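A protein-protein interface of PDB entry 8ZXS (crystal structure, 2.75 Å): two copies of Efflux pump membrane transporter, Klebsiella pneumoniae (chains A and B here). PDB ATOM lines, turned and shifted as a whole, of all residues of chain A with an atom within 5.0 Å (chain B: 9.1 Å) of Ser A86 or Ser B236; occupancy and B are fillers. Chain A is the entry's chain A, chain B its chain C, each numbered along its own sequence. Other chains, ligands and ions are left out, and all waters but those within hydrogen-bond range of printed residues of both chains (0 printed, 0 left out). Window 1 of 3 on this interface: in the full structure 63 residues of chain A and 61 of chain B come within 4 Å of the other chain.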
ATOM      1  N   ALA A  54      25.216 -23.038   6.579  1.00  0.00           N
ATOM      2  CA  ALA A  54      24.195 -22.027   6.333  1.00  0.00           C
ATOM      3  C   ALA A  54      22.800 -22.634   6.385  1.00  0.00           C
ATOM      4  O   ALA A  54      22.590 -23.778   5.964  1.00  0.00           O
ATOM      5  CB  ALA A  54      24.411 -21.353   4.981  1.00  0.00           C
ATOM      6  N   PRO A  56      19.127 -23.264   5.085  1.00  0.00           N
ATOM      7  CA  PRO A  56      18.415 -23.178   3.799  1.00  0.00           C
ATOM      8  C   PRO A  56      17.804 -21.811   3.543  1.00  0.00           C
ATOM      9  O   PRO A  56      17.821 -21.334   2.401  1.00  0.00           O
ATOM     10  CB  PRO A  56      17.341 -24.263   3.935  1.00  0.00           C
ATOM     11  CG  PRO A  56      17.963 -25.290   4.840  1.00  0.00           C
ATOM     12  CD  PRO A  56      18.911 -24.560   5.759  1.00  0.00           C
ATOM     13  N   ALA A  84      17.620 -25.797  -1.750  1.00  0.00           N
ATOM     14  CA  ALA A  84      18.628 -25.417  -0.760  1.00  0.00           C
ATOM     15  C   ALA A  84      18.405 -26.225   0.513  1.00  0.00           C
ATOM     16  O   ALA A  84      17.424 -26.002   1.231  1.00  0.00           O
ATOM     17  CB  ALA A  84      18.565 -23.919  -0.463  1.00  0.00           C
ATOM     18  N   GLY A  85      19.328 -27.143   0.807  1.00  0.00           N
ATOM     19  CA  GLY A  85      19.219 -27.998   1.968  1.00  0.00           C
ATOM     20  C   GLY A  85      20.047 -27.523   3.159  1.00  0.00           C
ATOM     21  O   GLY A  85      20.835 -26.585   3.080  1.00  0.00           O
ATOM     22  N   SER A  86      19.848 -28.208   4.283  1.00  0.00           N
ATOM     23  CA  SER A  86      20.557 -27.892   5.516  1.00  0.00           C
ATOM     24  C   SER A  86      21.979 -28.438   5.542  1.00  0.00           C
ATOM     25  O   SER A  86      22.707 -28.181   6.508  1.00  0.00           O
ATOM     26  CB  SER A  86      19.782 -28.420   6.723  1.00  0.00           C
ATOM     27  OG  SER A  86      19.587 -29.819   6.624  1.00  0.00           O
ATOM     28  N   ASP A  87      22.388 -29.190   4.523  1.00  0.00           N
ATOM     29  CA  ASP A  87      23.781 -29.582   4.361  1.00  0.00           C
ATOM     30  C   ASP A  87      24.625 -28.481   3.723  1.00  0.00           C
ATOM     31  O   ASP A  87      25.780 -28.735   3.361  1.00  0.00           O
ATOM     32  CB  ASP A  87      23.878 -30.863   3.529  1.00  0.00           C
ATOM     33  CG  ASP A  87      23.323 -30.695   2.124  1.00  0.00           C
ATOM     34  OD1 ASP A  87      22.518 -29.762   1.901  1.00  0.00           O
ATOM     35  OD2 ASP A  87      23.692 -31.501   1.242  1.00  0.00           O
ATOM     36  N   GLY A  88      24.069 -27.278   3.570  1.00  0.00           N
ATOM     37  CA  GLY A  88      24.801 -26.159   3.014  1.00  0.00           C
ATOM     38  C   GLY A  88      24.980 -26.159   1.511  1.00  0.00           C
ATOM     39  O   GLY A  88      25.811 -25.401   0.999  1.00  0.00           O
ATOM     40  N   ASN A 628      20.031 -33.748  -0.538  1.00  0.00           N
ATOM     41  CA  ASN A 628      20.256 -34.388   0.754  1.00  0.00           C
ATOM     42  C   ASN A 628      19.426 -33.685   1.818  1.00  0.00           C
ATOM     43  O   ASN A 628      19.633 -32.497   2.089  1.00  0.00           O
ATOM     44  CB  ASN A 628      21.735 -34.358   1.134  1.00  0.00           C
ATOM     45  CG  ASN A 628      22.565 -35.346   0.341  1.00  0.00           C
ATOM     46  OD1 ASN A 628      23.792 -35.242   0.297  1.00  0.00           O
ATOM     47  ND2 ASN A 628      21.904 -36.309  -0.290  1.00  0.00           N
ATOM     48  N   PRO A 630      17.975 -34.450   5.966  1.00  0.00           N
ATOM     49  CA  PRO A 630      18.336 -35.348   7.072  1.00  0.00           C
ATOM     50  C   PRO A 630      17.252 -36.352   7.448  1.00  0.00           C
ATOM     51  O   PRO A 630      17.574 -37.364   8.083  1.00  0.00           O
ATOM     52  CB  PRO A 630      18.636 -34.382   8.228  1.00  0.00           C
ATOM     53  CG  PRO A 630      17.871 -33.143   7.900  1.00  0.00           C
ATOM     54  CD  PRO A 630      17.799 -33.054   6.403  1.00  0.00           C
ATOM     55  N   PRO A 729      11.667 -28.309  12.983  1.00  0.00           N
ATOM     56  CA  PRO A 729      12.082 -27.494  14.132  1.00  0.00           C
ATOM     57  C   PRO A 729      13.483 -26.936  13.949  1.00  0.00           C
ATOM     58  O   PRO A 729      14.383 -27.609  13.441  1.00  0.00           O
ATOM     59  CB  PRO A 729      12.014 -28.477  15.307  1.00  0.00           C
ATOM     60  CG  PRO A 729      12.154 -29.821  14.674  1.00  0.00           C
ATOM     61  CD  PRO A 729      11.436 -29.713  13.362  1.00  0.00           C
ATOM     62  N   GLN A 730      13.666 -25.698  14.392  1.00  0.00           N
ATOM     63  CA  GLN A 730      14.901 -24.971  14.165  1.00  0.00           C
ATOM     64  C   GLN A 730      15.091 -23.984  15.308  1.00  0.00           C
ATOM     65  O   GLN A 730      14.211 -23.803  16.149  1.00  0.00           O
ATOM     66  CB  GLN A 730      14.874 -24.251  12.813  1.00  0.00           C
ATOM     67  CG  GLN A 730      15.154 -25.149  11.622  1.00  0.00           C
ATOM     68  CD  GLN A 730      14.789 -24.496  10.307  1.00  0.00           C
ATOM     69  OE1 GLN A 730      14.328 -23.354  10.278  1.00  0.00           O
ATOM     70  NE2 GLN A 730      15.008 -25.211   9.207  1.00  0.00           N
ATOM     71  N   LEU A 731      16.251 -23.335  15.330  1.00  0.00           N
ATOM     72  CA  LEU A 731      16.512 -22.277  16.291  1.00  0.00           C
ATOM     73  C   LEU A 731      16.886 -20.996  15.565  1.00  0.00           C
ATOM     74  O   LEU A 731      17.440 -21.026  14.462  1.00  0.00           O
ATOM     75  CB  LEU A 731      17.631 -22.645  17.272  1.00  0.00           C
ATOM     76  CG  LEU A 731      17.445 -23.911  18.103  1.00  0.00           C
ATOM     77  CD1 LEU A 731      18.754 -24.654  18.181  1.00  0.00           C
ATOM     78  CD2 LEU A 731      16.929 -23.567  19.487  1.00  0.00           C
ATOM     79  N   ASP A 818      12.845 -27.348   5.185  1.00  0.00           N
ATOM     80  CA  ASP A 818      14.135 -27.929   4.836  1.00  0.00           C
ATOM     81  C   ASP A 818      13.912 -29.141   3.939  1.00  0.00           C
ATOM     82  O   ASP A 818      13.477 -30.193   4.424  1.00  0.00           O
ATOM     83  CB  ASP A 818      14.909 -28.322   6.094  1.00  0.00           C
ATOM     84  CG  ASP A 818      16.220 -29.026   5.783  1.00  0.00           C
ATOM     85  OD1 ASP A 818      16.741 -29.716   6.687  1.00  0.00           O
ATOM     86  OD2 ASP A 818      16.732 -28.889   4.648  1.00  0.00           O
ATOM     87  N   ALA B 219      25.346 -20.453  10.853  1.00  0.00           N
ATOM     88  CA  ALA B 219      25.376 -20.824  12.264  1.00  0.00           C
ATOM     89  C   ALA B 219      25.215 -22.320  12.508  1.00  0.00           C
ATOM     90  O   ALA B 219      24.953 -22.717  13.652  1.00  0.00           O
ATOM     91  CB  ALA B 219      24.294 -20.063  13.040  1.00  0.00           C
ATOM     92  N   GLY B 220      25.348 -23.159  11.483  1.00  0.00           N
ATOM     93  CA  GLY B 220      25.352 -24.599  11.663  1.00  0.00           C
ATOM     94  C   GLY B 220      24.060 -25.120  12.264  1.00  0.00           C
ATOM     95  O   GLY B 220      22.970 -24.589  12.040  1.00  0.00           O
ATOM     96  N   GLN B 221      24.191 -26.189  13.047  1.00  0.00           N
ATOM     97  CA  GLN B 221      23.024 -26.854  13.607  1.00  0.00           C
ATOM     98  C   GLN B 221      23.421 -27.597  14.876  1.00  0.00           C
ATOM     99  O   GLN B 221      24.597 -27.891  15.106  1.00  0.00           O
ATOM    100  CB  GLN B 221      22.397 -27.812  12.591  1.00  0.00           C
ATOM    101  CG  GLN B 221      23.363 -28.829  12.035  1.00  0.00           C
ATOM    102  CD  GLN B 221      23.826 -28.485  10.644  1.00  0.00           C
ATOM    103  OE1 GLN B 221      24.290 -27.374  10.390  1.00  0.00           O
ATOM    104  NE2 GLN B 221      23.710 -29.443   9.728  1.00  0.00           N
ATOM    105  N   LEU B 222      22.421 -27.887  15.705  1.00  0.00           N
ATOM    106  CA  LEU B 222      22.622 -28.695  16.899  1.00  0.00           C
ATOM    107  C   LEU B 222      22.419 -30.165  16.564  1.00  0.00           C
ATOM    108  O   LEU B 222      21.631 -30.518  15.684  1.00  0.00           O
ATOM    109  CB  LEU B 222      21.670 -28.274  18.019  1.00  0.00           C
ATOM    110  CG  LEU B 222      21.852 -26.867  18.599  1.00  0.00           C
ATOM    111  CD1 LEU B 222      21.050 -26.711  19.874  1.00  0.00           C
ATOM    112  CD2 LEU B 222      23.317 -26.555  18.862  1.00  0.00           C
ATOM    113  N   GLY B 223      23.150 -31.025  17.267  1.00  0.00           N
ATOM    114  CA  GLY B 223      23.022 -32.450  17.034  1.00  0.00           C
ATOM    115  C   GLY B 223      23.665 -32.958  15.765  1.00  0.00           C
ATOM    116  O   GLY B 223      23.266 -34.011  15.263  1.00  0.00           O
ATOM    117  N   ALA B 224      24.656 -32.247  15.232  1.00  0.00           N
ATOM    118  CA  ALA B 224      25.336 -32.667  14.017  1.00  0.00           C
ATOM    119  C   ALA B 224      26.567 -33.518  14.338  1.00  0.00           C
ATOM    120  O   ALA B 224      27.052 -33.566  15.471  1.00  0.00           O
ATOM    121  CB  ALA B 224      25.729 -31.452  13.179  1.00  0.00           C
ATOM    122  N   PHE B 233      17.950 -36.001  17.047  1.00  0.00           N
ATOM    123  CA  PHE B 233      17.399 -34.850  16.348  1.00  0.00           C
ATOM    124  C   PHE B 233      18.501 -34.026  15.694  1.00  0.00           C
ATOM    125  O   PHE B 233      19.639 -33.981  16.173  1.00  0.00           O
ATOM    126  CB  PHE B 233      16.589 -33.959  17.304  1.00  0.00           C
ATOM    127  CG  PHE B 233      15.165 -34.402  17.490  1.00  0.00           C
ATOM    128  CD1 PHE B 233      14.815 -35.739  17.389  1.00  0.00           C
ATOM    129  CD2 PHE B 233      14.168 -33.477  17.742  1.00  0.00           C
ATOM    130  CE1 PHE B 233      13.509 -36.147  17.553  1.00  0.00           C
ATOM    131  CE2 PHE B 233      12.861 -33.877  17.899  1.00  0.00           C
ATOM    132  CZ  PHE B 233      12.529 -35.215  17.807  1.00  0.00           C
ATOM    133  N   LEU B 234      18.143 -33.371  14.589  1.00  0.00           N
ATOM    134  CA  LEU B 234      19.012 -32.432  13.885  1.00  0.00           C
ATOM    135  C   LEU B 234      18.271 -31.107  13.762  1.00  0.00           C
ATOM    136  O   LEU B 234      17.294 -31.010  13.012  1.00  0.00           O
ATOM    137  CB  LEU B 234      19.398 -32.962  12.504  1.00  0.00           C
ATOM    138  CG  LEU B 234      20.558 -32.259  11.801  1.00  0.00           C
ATOM    139  CD1 LEU B 234      21.559 -31.757  12.819  1.00  0.00           C
ATOM    140  CD2 LEU B 234      21.228 -33.201  10.820  1.00  0.00           C
ATOM    141  N   ILE B 235      18.734 -30.088  14.481  1.00  0.00           N
ATOM    142  CA  ILE B 235      18.035 -28.809  14.597  1.00  0.00           C
ATOM    143  C   ILE B 235      18.909 -27.732  13.970  1.00  0.00           C
ATOM    144  O   ILE B 235      19.943 -27.360  14.539  1.00  0.00           O
ATOM    145  CB  ILE B 235      17.716 -28.462  16.058  1.00  0.00           C
ATOM    146  CG1 ILE B 235      16.740 -29.465  16.686  1.00  0.00           C
ATOM    147  CG2 ILE B 235      17.145 -27.058  16.145  1.00  0.00           C
ATOM    148  CD1 ILE B 235      15.755 -30.116  15.711  1.00  0.00           C
ATOM    149  N   SER B 236      18.486 -27.206  12.819  1.00  0.00           N
ATOM    150  CA  SER B 236      19.224 -26.130  12.164  1.00  0.00           C
ATOM    151  C   SER B 236      19.176 -24.850  12.991  1.00  0.00           C
ATOM    152  O   SER B 236      18.204 -24.572  13.698  1.00  0.00           O
ATOM    153  CB  SER B 236      18.661 -25.848  10.768  1.00  0.00           C
ATOM    154  OG  SER B 236      19.014 -26.850   9.831  1.00  0.00           O
ATOM    155  N   ILE B 237      20.240 -24.060  12.881  1.00  0.00           N
ATOM    156  CA  ILE B 237      20.381 -22.806  13.612  1.00  0.00           C
ATOM    157  C   ILE B 237      20.445 -21.675  12.602  1.00  0.00           C
ATOM    158  O   ILE B 237      21.250 -21.715  11.663  1.00  0.00           O
ATOM    159  CB  ILE B 237      21.630 -22.799  14.514  1.00  0.00           C
ATOM    160  CG1 ILE B 237      21.658 -24.034  15.413  1.00  0.00           C
ATOM    161  CG2 ILE B 237      21.667 -21.544  15.375  1.00  0.00           C
ATOM    162  CD1 ILE B 237      22.939 -24.164  16.192  1.00  0.00           C
ATOM    163  N   ASN B 238      19.594 -20.676  12.791  1.00  0.00           N
ATOM    164  CA  ASN B 238      19.572 -19.500  11.938  1.00  0.00           C
ATOM    165  C   ASN B 238      19.965 -18.293  12.766  1.00  0.00           C
ATOM    166  O   ASN B 238      19.337 -18.004  13.787  1.00  0.00           O
ATOM    167  CB  ASN B 238      18.194 -19.292  11.303  1.00  0.00           C
ATOM    168  CG  ASN B 238      17.927 -17.833  10.946  1.00  0.00           C
ATOM    169  OD1 ASN B 238      17.467 -17.044  11.776  1.00  0.00           O
ATOM    170  ND2 ASN B 238      18.257 -17.461   9.712  1.00  0.00           N
ATOM    171  N   ALA B 239      21.008 -17.601  12.328  1.00  0.00           N
ATOM    172  CA  ALA B 239      21.390 -16.311  12.873  1.00  0.00           C
ATOM    173  C   ALA B 239      21.197 -15.273  11.780  1.00  0.00           C
ATOM    174  O   ALA B 239      21.599 -15.498  10.634  1.00  0.00           O
ATOM    175  CB  ALA B 239      22.838 -16.329  13.354  1.00  0.00           C
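OG of Ser A86 is in hydrogen-bond range of OD1 of Asp A818, 2.8 Å away.
N of Ile B237 is in hydrogen-bond range of O of Gly B220.
The backbone NH (N) of Leu B222 sits at hydrogen-bond distance from the backbone carbonyl oxygen (O) of Ile B235.
Of the 13 printed residues of chain A, 5 touch a printed residue of chain B.
Printed residues of chain A that touch a printed residue of chain B: Ser A86, Pro A630, Pro A729, Gln A730 and Leu A731.
Hydrophobic or aromatic side chains of chain A that line the printed part of chain B: Pro A630, Pro A729 and Leu A731.
Among the printed residues, 11 pairs touch across the chains.
Among the printed residues, no Asp or Glu carboxylate lies within 4 Å of a Lys or Arg side-chain nitrogen of the other chain.
Among the printed residues, merely in contact across the chains: Gln A730 with Ser B236, Leu A731 with Leu B222, Leu A731 with Ile B235, Leu A731 with Ile B237, Ser A86 with Ser B236, Ser A86 with Gln B221, Gln A730 with Ile B235, Pro A729 with Ile B235 and Pro A630 with Leu B234.
The backbone NH of Leu A731 is in hydrogen-bond range of the backbone carbonyl oxygen of Ser B236, at 2.8 Å.
The backbone NH (N) of Asn B238 sits at hydrogen-bond distance from the backbone carbonyl oxygen (O) of Leu A731, 2.7 Å away.
No position is printed for both chains.
Of the 11 pairs that touch across the chains among the printed residues, none has its exchanged pair printed and touching as well.
Of chain B, only Gln B221 and Ser B236 come within 4 Å of Ser A86.
Of chain A, only Ser A86 (3.6 Å), Gln A730 (3.4 Å) and Leu A731 (2.8 Å) come within 4 Å of Ser B236.
No residue of chain B comes within 4 Å of Gly A85.
Of the printed residues of chain B, Pro A630 touches Leu B234 (3.9 Å).
Printed residues of chain A within 4 Å of Leu B222: Leu A731 (3.5 Å).
Gly A88 touches none of the printed residues of chain B.
Pro A56 touches none of the printed residues of chain B.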
